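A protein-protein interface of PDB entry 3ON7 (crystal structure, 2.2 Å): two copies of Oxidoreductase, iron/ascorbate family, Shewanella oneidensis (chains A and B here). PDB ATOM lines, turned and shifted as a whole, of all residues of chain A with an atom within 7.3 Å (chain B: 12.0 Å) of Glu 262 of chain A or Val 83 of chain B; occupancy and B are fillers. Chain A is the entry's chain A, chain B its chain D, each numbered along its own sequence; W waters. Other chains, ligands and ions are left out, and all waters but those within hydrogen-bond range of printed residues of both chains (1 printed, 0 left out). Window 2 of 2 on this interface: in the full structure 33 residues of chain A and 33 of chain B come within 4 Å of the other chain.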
ATOM      1  N   LYS A 135     -32.229  -6.822 -13.368  1.00  0.00           N
ATOM      2  CA  LYS A 135     -31.739  -5.460 -13.655  1.00  0.00           C
ATOM      3  C   LYS A 135     -32.280  -4.378 -12.699  1.00  0.00           C
ATOM      4  O   LYS A 135     -31.836  -3.230 -12.758  1.00  0.00           O
ATOM      5  CB  LYS A 135     -32.106  -5.067 -15.090  1.00  0.00           C
ATOM      6  CG  LYS A 135     -31.443  -5.922 -16.161  1.00  0.00           C
ATOM      7  CD  LYS A 135     -31.910  -5.537 -17.567  1.00  0.00           C
ATOM      8  CE  LYS A 135     -31.194  -6.354 -18.663  1.00  0.00           C
ATOM      9  NZ  LYS A 135     -29.717  -6.164 -18.628  1.00  0.00           N
ATOM     10  N   GLU A 220     -35.915   2.624 -18.789  1.00  0.00           N
ATOM     11  CA  GLU A 220     -34.476   2.537 -18.617  1.00  0.00           C
ATOM     12  C   GLU A 220     -34.091   1.446 -17.634  1.00  0.00           C
ATOM     13  O   GLU A 220     -33.120   0.723 -17.862  1.00  0.00           O
ATOM     14  CB  GLU A 220     -33.949   3.910 -18.149  1.00  0.00           C
ATOM     15  CG  GLU A 220     -32.493   3.988 -17.803  1.00  0.00           C
ATOM     16  CD  GLU A 220     -31.577   3.669 -18.954  1.00  0.00           C
ATOM     17  OE1 GLU A 220     -32.025   3.776 -20.127  1.00  0.00           O
ATOM     18  OE2 GLU A 220     -30.391   3.327 -18.665  1.00  0.00           O
ATOM     19  N   VAL A 258     -31.807   6.257  -6.701  1.00  0.00           N
ATOM     20  CA  VAL A 258     -32.038   4.925  -7.237  1.00  0.00           C
ATOM     21  C   VAL A 258     -31.221   4.695  -8.501  1.00  0.00           C
ATOM     22  O   VAL A 258     -31.255   5.475  -9.456  1.00  0.00           O
ATOM     23  CB  VAL A 258     -33.521   4.674  -7.543  1.00  0.00           C
ATOM     24  CG1 VAL A 258     -33.697   3.360  -8.320  1.00  0.00           C
ATOM     25  CG2 VAL A 258     -34.325   4.659  -6.245  1.00  0.00           C
ATOM     26  N   VAL A 259     -30.493   3.591  -8.503  1.00  0.00           N
ATOM     27  CA  VAL A 259     -29.720   3.178  -9.658  1.00  0.00           C
ATOM     28  C   VAL A 259     -30.693   2.516 -10.609  1.00  0.00           C
ATOM     29  O   VAL A 259     -31.252   1.485 -10.279  1.00  0.00           O
ATOM     30  CB  VAL A 259     -28.644   2.160  -9.277  1.00  0.00           C
ATOM     31  CG1 VAL A 259     -27.969   1.652 -10.538  1.00  0.00           C
ATOM     32  CG2 VAL A 259     -27.632   2.778  -8.250  1.00  0.00           C
ATOM     33  N   LEU A 260     -30.886   3.124 -11.777  1.00  0.00           N
ATOM     34  CA  LEU A 260     -31.777   2.596 -12.817  1.00  0.00           C
ATOM     35  C   LEU A 260     -31.073   1.553 -13.676  1.00  0.00           C
ATOM     36  O   LEU A 260     -31.664   0.556 -14.035  1.00  0.00           O
ATOM     37  CB  LEU A 260     -32.308   3.723 -13.714  1.00  0.00           C
ATOM     38  CG  LEU A 260     -33.152   4.805 -13.045  1.00  0.00           C
ATOM     39  CD1 LEU A 260     -33.401   5.964 -14.024  1.00  0.00           C
ATOM     40  CD2 LEU A 260     -34.470   4.267 -12.496  1.00  0.00           C
ATOM     41  N   SER A 261     -29.813   1.795 -14.010  1.00  0.00           N
ATOM     42  CA  SER A 261     -29.058   0.893 -14.871  1.00  0.00           C
ATOM     43  C   SER A 261     -27.562   1.083 -14.647  1.00  0.00           C
ATOM     44  O   SER A 261     -27.157   1.823 -13.757  1.00  0.00           O
ATOM     45  CB  SER A 261     -29.398   1.212 -16.318  1.00  0.00           C
ATOM     46  OG  SER A 261     -28.832   2.461 -16.650  1.00  0.00           O
ATOM     47  N   GLU A 262     -26.736   0.450 -15.467  1.00  0.00           N
ATOM     48  CA  GLU A 262     -25.297   0.680 -15.403  1.00  0.00           C
ATOM     49  C   GLU A 262     -24.917   2.109 -15.814  1.00  0.00           C
ATOM     50  O   GLU A 262     -23.848   2.578 -15.455  1.00  0.00           O
ATOM     51  CB  GLU A 262     -24.547  -0.333 -16.283  1.00  0.00           C
ATOM     52  CG  GLU A 262     -24.446  -1.734 -15.655  1.00  0.00           C
ATOM     53  N   ARG A 263     -25.811   2.787 -16.539  1.00  0.00           N
ATOM     54  CA  ARG A 263     -25.534   4.107 -17.114  1.00  0.00           C
ATOM     55  C   ARG A 263     -26.055   5.237 -16.234  1.00  0.00           C
ATOM     56  O   ARG A 263     -25.471   6.304 -16.206  1.00  0.00           O
ATOM     57  CB  ARG A 263     -26.167   4.261 -18.513  1.00  0.00           C
ATOM     58  CG  ARG A 263     -25.455   3.558 -19.685  1.00  0.00           C
ATOM     59  CD  ARG A 263     -26.238   3.737 -21.010  1.00  0.00           C
ATOM     60  NE  ARG A 263     -26.436   5.152 -21.356  1.00  0.00           N
ATOM     61  CZ  ARG A 263     -26.811   5.596 -22.559  1.00  0.00           C
ATOM     62  NH1 ARG A 263     -27.041   4.746 -23.552  1.00  0.00           N
ATOM     63  NH2 ARG A 263     -26.953   6.896 -22.771  1.00  0.00           N
ATOM     64  N   TYR A 264     -27.170   5.017 -15.516  1.00  0.00           N
ATOM     65  CA  TYR A 264     -27.829   6.100 -14.755  1.00  0.00           C
ATOM     66  C   TYR A 264     -28.425   5.743 -13.408  1.00  0.00           C
ATOM     67  O   TYR A 264     -28.918   4.626 -13.204  1.00  0.00           O
ATOM     68  CB  TYR A 264     -29.032   6.668 -15.514  1.00  0.00           C
ATOM     69  CG  TYR A 264     -28.769   7.210 -16.874  1.00  0.00           C
ATOM     70  CD1 TYR A 264     -28.289   8.494 -17.054  1.00  0.00           C
ATOM     71  CD2 TYR A 264     -29.040   6.454 -17.983  1.00  0.00           C
ATOM     72  CE1 TYR A 264     -28.060   8.979 -18.318  1.00  0.00           C
ATOM     73  CE2 TYR A 264     -28.834   6.931 -19.226  1.00  0.00           C
ATOM     74  CZ  TYR A 264     -28.351   8.185 -19.401  1.00  0.00           C
ATOM     75  OH  TYR A 264     -28.154   8.619 -20.685  1.00  0.00           O
ATOM     76  N   THR A 265     -28.415   6.761 -12.537  1.00  0.00           N
ATOM     77  CA  THR A 265     -29.312   6.876 -11.394  1.00  0.00           C
ATOM     78  C   THR A 265     -30.438   7.772 -11.858  1.00  0.00           C
ATOM     79  O   THR A 265     -30.300   8.434 -12.868  1.00  0.00           O
ATOM     80  CB  THR A 265     -28.635   7.519 -10.177  1.00  0.00           C
ATOM     81  OG1 THR A 265     -28.179   8.858 -10.487  1.00  0.00           O
ATOM     82  CG2 THR A 265     -27.456   6.684  -9.718  1.00  0.00           C
ATOM     83  N   SER A 268     -29.149  11.306 -12.170  1.00  0.00           N
ATOM     84  CA  SER A 268     -28.247  11.622 -13.281  1.00  0.00           C
ATOM     85  C   SER A 268     -29.010  11.542 -14.598  1.00  0.00           C
ATOM     86  O   SER A 268     -28.676  12.237 -15.554  1.00  0.00           O
ATOM     87  CB  SER A 268     -27.012  10.705 -13.289  1.00  0.00           C
ATOM     88  OG  SER A 268     -27.325   9.407 -13.755  1.00  0.00           O
ATOM     89  N   PHE B  70     -18.191  17.773 -19.194  1.00  0.00           N
ATOM     90  CA  PHE B  70     -18.997  16.766 -18.497  1.00  0.00           C
ATOM     91  C   PHE B  70     -18.412  15.364 -18.697  1.00  0.00           C
ATOM     92  O   PHE B  70     -18.518  14.830 -19.786  1.00  0.00           O
ATOM     93  CB  PHE B  70     -20.408  16.773 -19.065  1.00  0.00           C
ATOM     94  CG  PHE B  70     -21.160  18.025 -18.772  1.00  0.00           C
ATOM     95  CD1 PHE B  70     -21.047  19.124 -19.598  1.00  0.00           C
ATOM     96  CD2 PHE B  70     -21.991  18.109 -17.663  1.00  0.00           C
ATOM     97  CE1 PHE B  70     -21.727  20.281 -19.312  1.00  0.00           C
ATOM     98  CE2 PHE B  70     -22.666  19.258 -17.391  1.00  0.00           C
ATOM     99  CZ  PHE B  70     -22.545  20.340 -18.217  1.00  0.00           C
ATOM    100  N   PRO B  71     -17.826  14.761 -17.652  1.00  0.00           N
ATOM    101  CA  PRO B  71     -17.293  13.389 -17.755  1.00  0.00           C
ATOM    102  C   PRO B  71     -18.354  12.294 -17.734  1.00  0.00           C
ATOM    103  O   PRO B  71     -19.484  12.533 -17.325  1.00  0.00           O
ATOM    104  CB  PRO B  71     -16.386  13.254 -16.524  1.00  0.00           C
ATOM    105  CG  PRO B  71     -16.882  14.270 -15.548  1.00  0.00           C
ATOM    106  CD  PRO B  71     -17.465  15.401 -16.371  1.00  0.00           C
ATOM    107  N   ALA B  72     -17.972  11.099 -18.188  1.00  0.00           N
ATOM    108  CA  ALA B  72     -18.854   9.934 -18.217  1.00  0.00           C
ATOM    109  C   ALA B  72     -19.354   9.552 -16.810  1.00  0.00           C
ATOM    110  O   ALA B  72     -20.508   9.098 -16.631  1.00  0.00           O
ATOM    111  CB  ALA B  72     -18.130   8.750 -18.875  1.00  0.00           C
ATOM    112  N   SER B  73     -18.493   9.739 -15.813  1.00  0.00           N
ATOM    113  CA  SER B  73     -18.825   9.385 -14.427  1.00  0.00           C
ATOM    114  C   SER B  73     -18.399  10.474 -13.430  1.00  0.00           C
ATOM    115  O   SER B  73     -17.461  11.214 -13.684  1.00  0.00           O
ATOM    116  CB  SER B  73     -18.147   8.060 -14.081  1.00  0.00           C
ATOM    117  OG  SER B  73     -18.387   7.708 -12.740  1.00  0.00           O
ATOM    118  N   ILE B  74     -19.086  10.559 -12.288  1.00  0.00           N
ATOM    119  CA  ILE B  74     -18.704  11.505 -11.220  1.00  0.00           C
ATOM    120  C   ILE B  74     -17.693  10.880 -10.235  1.00  0.00           C
ATOM    121  O   ILE B  74     -18.057  10.227  -9.249  1.00  0.00           O
ATOM    122  CB  ILE B  74     -19.940  12.030 -10.454  1.00  0.00           C
ATOM    123  N   HIS B  81     -23.595   1.304  -5.998  1.00  0.00           N
ATOM    124  CA  HIS B  81     -22.183   1.639  -5.841  1.00  0.00           C
ATOM    125  C   HIS B  81     -21.789   2.807  -6.761  1.00  0.00           C
ATOM    126  O   HIS B  81     -21.548   3.934  -6.291  1.00  0.00           O
ATOM    127  CB  HIS B  81     -21.308   0.411  -6.139  1.00  0.00           C
ATOM    128  N   THR B  82     -21.763   2.530  -8.072  1.00  0.00           N
ATOM    129  CA  THR B  82     -21.272   3.480  -9.085  1.00  0.00           C
ATOM    130  C   THR B  82     -21.833   3.236 -10.519  1.00  0.00           C
ATOM    131  O   THR B  82     -22.144   2.103 -10.915  1.00  0.00           O
ATOM    132  CB  THR B  82     -19.729   3.474  -9.106  1.00  0.00           C
ATOM    133  OG1 THR B  82     -19.262   4.603  -9.861  1.00  0.00           O
ATOM    134  CG2 THR B  82     -19.177   2.124  -9.684  1.00  0.00           C
ATOM    135  N   VAL B  83     -21.900   4.316 -11.292  1.00  0.00           N
ATOM    136  CA  VAL B  83     -22.695   4.399 -12.514  1.00  0.00           C
ATOM    137  C   VAL B  83     -21.906   5.177 -13.562  1.00  0.00           C
ATOM    138  O   VAL B  83     -21.203   6.109 -13.201  1.00  0.00           O
ATOM    139  CB  VAL B  83     -24.041   5.107 -12.177  1.00  0.00           C
ATOM    140  CG1 VAL B  83     -24.444   6.125 -13.218  1.00  0.00           C
ATOM    141  CG2 VAL B  83     -25.146   4.074 -11.911  1.00  0.00           C
ATOM    142  N   LYS B  84     -22.015   4.817 -14.844  1.00  0.00           N
ATOM    143  CA  LYS B  84     -21.162   5.423 -15.895  1.00  0.00           C
ATOM    144  C   LYS B  84     -21.814   5.475 -17.278  1.00  0.00           C
ATOM    145  O   LYS B  84     -22.048   4.437 -17.885  1.00  0.00           O
ATOM    146  CB  LYS B  84     -19.852   4.636 -15.999  1.00  0.00           C
ATOM    147  CG  LYS B  84     -18.905   5.042 -17.138  1.00  0.00           C
ATOM    148  CD  LYS B  84     -17.665   4.132 -17.137  1.00  0.00           C
ATOM    149  CE  LYS B  84     -16.806   4.292 -18.400  1.00  0.00           C
ATOM    150  NZ  LYS B  84     -15.551   3.477 -18.344  1.00  0.00           N
ATOM    151  N   ASP B  85     -22.056   6.677 -17.792  1.00  0.00           N
ATOM    152  CA  ASP B  85     -22.639   6.848 -19.136  1.00  0.00           C
ATOM    153  C   ASP B  85     -21.640   6.411 -20.234  1.00  0.00           C
ATOM    154  O   ASP B  85     -20.448   6.181 -19.964  1.00  0.00           O
ATOM    155  CB  ASP B  85     -23.116   8.303 -19.347  1.00  0.00           C
ATOM    156  CG  ASP B  85     -24.233   8.442 -20.412  1.00  0.00           C
ATOM    157  OD1 ASP B  85     -24.499   7.490 -21.171  1.00  0.00           O
ATOM    158  OD2 ASP B  85     -24.857   9.523 -20.483  1.00  0.00           O
ATOM    159  N   ILE B  86     -22.139   6.281 -21.460  1.00  0.00           N
ATOM    160  CA  ILE B  86     -21.330   5.804 -22.585  1.00  0.00           C
ATOM    161  C   ILE B  86     -20.761   6.960 -23.404  1.00  0.00           C
ATOM    162  O   ILE B  86     -20.096   6.737 -24.426  1.00  0.00           O
ATOM    163  CB  ILE B  86     -22.142   4.860 -23.507  1.00  0.00           C
ATOM    164  CG1 ILE B  86     -23.379   5.572 -24.078  1.00  0.00           C
ATOM    165  CG2 ILE B  86     -22.522   3.605 -22.743  1.00  0.00           C
ATOM    166  CD1 ILE B  86     -24.158   4.743 -25.037  1.00  0.00           C
ATOM    167  N   LYS B  87     -21.020   8.187 -22.946  1.00  0.00           N
ATOM    168  CA  LYS B  87     -20.477   9.372 -23.567  1.00  0.00           C
ATOM    169  C   LYS B  87     -19.997  10.384 -22.517  1.00  0.00           C
ATOM    170  O   LYS B  87     -20.375  10.335 -21.356  1.00  0.00           O
ATOM    171  CB  LYS B  87     -21.545  10.035 -24.445  1.00  0.00           C
ATOM    172  CG  LYS B  87     -22.751  10.588 -23.656  1.00  0.00           C
ATOM    173  CD  LYS B  87     -23.936  10.935 -24.583  1.00  0.00           C
ATOM    174  CE  LYS B  87     -25.155  11.530 -23.839  1.00  0.00           C
ATOM    175  NZ  LYS B  87     -25.971  10.545 -23.044  1.00  0.00           N
ATOM    176  N   GLU B  88     -19.180  11.314 -22.985  1.00  0.00           N
ATOM    177  CA  GLU B  88     -18.730  12.467 -22.232  1.00  0.00           C
ATOM    178  C   GLU B  88     -18.884  13.603 -23.230  1.00  0.00           C
ATOM    179  O   GLU B  88     -18.968  13.348 -24.440  1.00  0.00           O
ATOM    180  CB  GLU B  88     -17.273  12.281 -21.779  1.00  0.00           C
ATOM    181  CG  GLU B  88     -16.238  12.225 -22.927  1.00  0.00           C
ATOM    182  CD  GLU B  88     -14.789  11.911 -22.489  1.00  0.00           C
ATOM    183  OE1 GLU B  88     -14.455  11.933 -21.286  1.00  0.00           O
ATOM    184  OE2 GLU B  88     -13.974  11.612 -23.374  1.00  0.00           O
ATOM    185  N   TYR B  89     -18.936  14.845 -22.760  1.00  0.00           N
ATOM    186  CA  TYR B  89     -19.123  15.960 -23.691  1.00  0.00           C
ATOM    187  C   TYR B  89     -18.693  17.314 -23.154  1.00  0.00           C
ATOM    188  O   TYR B  89     -18.360  17.462 -21.971  1.00  0.00           O
ATOM    189  CB  TYR B  89     -20.583  16.025 -24.140  1.00  0.00           C
ATOM    190  CG  TYR B  89     -21.584  16.021 -23.000  1.00  0.00           C
ATOM    191  CD1 TYR B  89     -22.026  14.818 -22.436  1.00  0.00           C
ATOM    192  CD2 TYR B  89     -22.095  17.209 -22.497  1.00  0.00           C
ATOM    193  CE1 TYR B  89     -22.941  14.803 -21.403  1.00  0.00           C
ATOM    194  CE2 TYR B  89     -23.013  17.205 -21.456  1.00  0.00           C
ATOM    195  CZ  TYR B  89     -23.432  16.002 -20.912  1.00  0.00           C
ATOM    196  OH  TYR B  89     -24.348  15.998 -19.875  1.00  0.00           O
ATOM    197  N   MET B 160     -15.101   1.330 -26.586  1.00  0.00           N
ATOM    198  CA  MET B 160     -15.510   0.269 -25.694  1.00  0.00           C
ATOM    199  C   MET B 160     -14.254  -0.502 -25.346  1.00  0.00           C
ATOM    200  O   MET B 160     -13.500  -0.895 -26.241  1.00  0.00           O
ATOM    201  CB  MET B 160     -16.510  -0.641 -26.397  1.00  0.00           C
ATOM    202  CG  MET B 160     -17.789   0.096 -26.785  1.00  0.00           C
ATOM    203  SD  MET B 160     -19.184  -0.257 -25.521  1.00  0.00           S
ATOM    204  CE  MET B 160     -20.045   1.474 -25.427  1.00  0.00           C
ATOM    205  N   ASP B 163     -14.176  -6.188 -22.423  1.00  0.00           N
ATOM    206  CA  ASP B 163     -15.395  -6.978 -22.603  1.00  0.00           C
ATOM    207  C   ASP B 163     -16.628  -6.125 -22.298  1.00  0.00           C
ATOM    208  O   ASP B 163     -17.639  -6.630 -21.818  1.00  0.00           O
ATOM    209  CB  ASP B 163     -15.360  -8.237 -21.720  1.00  0.00           C
ATOM    210  N   GLU B 164     -16.529  -4.824 -22.564  1.00  0.00           N
ATOM    211  CA  GLU B 164     -17.711  -3.967 -22.604  1.00  0.00           C
ATOM    212  C   GLU B 164     -18.469  -4.326 -23.886  1.00  0.00           C
ATOM    213  O   GLU B 164     -17.856  -4.595 -24.925  1.00  0.00           O
ATOM    214  CB  GLU B 164     -17.339  -2.475 -22.572  1.00  0.00           C
ATOM    215  CG  GLU B 164     -16.936  -1.939 -21.179  1.00  0.00           C
ATOM    216  CD  GLU B 164     -16.728  -0.414 -21.142  1.00  0.00           C
ATOM    217  OE1 GLU B 164     -15.907   0.104 -21.933  1.00  0.00           O
ATOM    218  OE2 GLU B 164     -17.376   0.263 -20.308  1.00  0.00           O
ATOM    219  N   GLU B 165     -19.797  -4.368 -23.792  1.00  0.00           N
ATOM    220  CA  GLU B 165     -20.647  -4.731 -24.926  1.00  0.00           C
ATOM    221  C   GLU B 165     -21.277  -3.457 -25.484  1.00  0.00           C
ATOM    222  O   GLU B 165     -21.487  -2.490 -24.753  1.00  0.00           O
ATOM    223  CB  GLU B 165     -21.724  -5.747 -24.493  1.00  0.00           C
ATOM    224  N   MET B 166     -21.551  -3.454 -26.785  1.00  0.00           N
ATOM    225  CA  MET B 166     -22.132  -2.292 -27.461  1.00  0.00           C
ATOM    226  C   MET B 166     -23.619  -2.533 -27.691  1.00  0.00           C
ATOM    227  O   MET B 166     -24.001  -3.478 -28.376  1.00  0.00           O
ATOM    228  CB  MET B 166     -21.427  -2.038 -28.804  1.00  0.00           C
ATOM    229  CG  MET B 166     -21.605  -0.629 -29.338  1.00  0.00           C
ATOM    230  SD  MET B 166     -20.817  -0.324 -31.095  1.00  0.00           S
ATOM    231  CE  MET B 166     -20.018   1.394 -30.706  1.00  0.00           C
ATOM    232  N   GLY B 167     -24.452  -1.678 -27.114  1.00  0.00           N
ATOM    233  CA  GLY B 167     -25.889  -1.749 -27.332  1.00  0.00           C
ATOM    234  C   GLY B 167     -26.261  -1.481 -28.778  1.00  0.00           C
ATOM    235  O   GLY B 167     -25.472  -0.906 -29.535  1.00  0.00           O
HETATM  236  O   HOH W   1     -26.338   8.825 -25.444  1.00  0.00           O
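O of Glu 262 of chain A lies within hydrogen-bond range of N of Lys 84 of chain B (3.0 Å). The guanidinium group (NH2) of Arg 263 of chain A is in salt-bridge range of the side-chain carboxylate (OD1) of Asp 85 of chain B. OD2 of Asp 85 of chain B sits at hydrogen-bond distance from OH of Tyr 264 of chain A (3.4 Å).
The backbone carbonyl oxygen (O) of Ala 72 of chain B lies within hydrogen-bond range of the backbone NH (N) of Asp 85 of chain B. The guanidinium group of Arg 263 of chain A sits at hydrogen-bond distance from the side-chain hydroxyl of Tyr 264 of chain A, 3.0 Å away. OG of Ser 261 of chain A sits at hydrogen-bond distance from N of Tyr 264 of chain A (3.3 Å). OG of Ser 261 of chain A sits at hydrogen-bond distance from N of Arg 263 of chain A, at 3.0 Å. The side-chain carboxylate (OE2) of Glu 220 of chain A sits at hydrogen-bond distance from the side-chain hydroxyl (OG) of Ser 261 of chain A. The side-chain amino group (NZ) of Lys 87 of chain B is in salt-bridge range of the side-chain carboxylate (OD2) of Asp 85 of chain B.
Among the printed residues, pairs that only touch across the chains: Arg 263 of chain A with Val 83 of chain B (3.2 Å), Arg 263 of chain A with Ile 86 of chain B (3.2 Å), Ser 261 of chain A with Val 83 of chain B (3.5 Å), Arg 263 of chain A with Lys 84 of chain B (3.6 Å), Glu 262 of chain A with Val 83 of chain B (3.6 Å), Tyr 264 of chain A with Val 83 of chain B (3.7 Å), Tyr 264 of chain A with Lys 87 of chain B (3.7 Å), Arg 263 of chain A with Lys 87 of chain B (3.8 Å) and Val 259 of chain A with Val 83 of chain B (3.96 Å).
Glu 262 of chain A touches just these residues of chain B: Val 83 (3.6 Å) and Lys 84 (3.0 Å). Val 259 of chain A touches just one residue of chain B: Val 83. Ser 261 of chain A touches just one residue of chain B: Val 83. No residue of chain B comes within 4 Å of Ser 268 of chain A. Of the printed residues of chain A, Asp 85 of chain B touches Arg 263 and Tyr 264. Of the printed residues of chain A, Ile 86 of chain B touches Arg 263 (3.2 Å). Thr 82 of chain B touches none of the printed residues of chain A. The nearest residue of chain B that does not touch Glu 262 of chain A is Thr 82 of chain B (4.9 Å). The nearest printed residue of chain A that does not touch Asp 85 of chain B is Glu 262 of chain A (5.0 Å).
Of the 11 printed residues of chain A, 5 touch a printed residue of chain B. Hydrophobic or aromatic side chains of chain B that line the printed part of chain A: Val 83 and Ile 86. Among the printed residues, 12 pairs touch across the chains.
No position is printed for both chains.
Water W1 bridges the side-chain amino group (NZ) of Lys 87 of chain B (3.0 Å) and the guanidinium group (NH2) of Arg 263 of chain A (3.4 Å).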
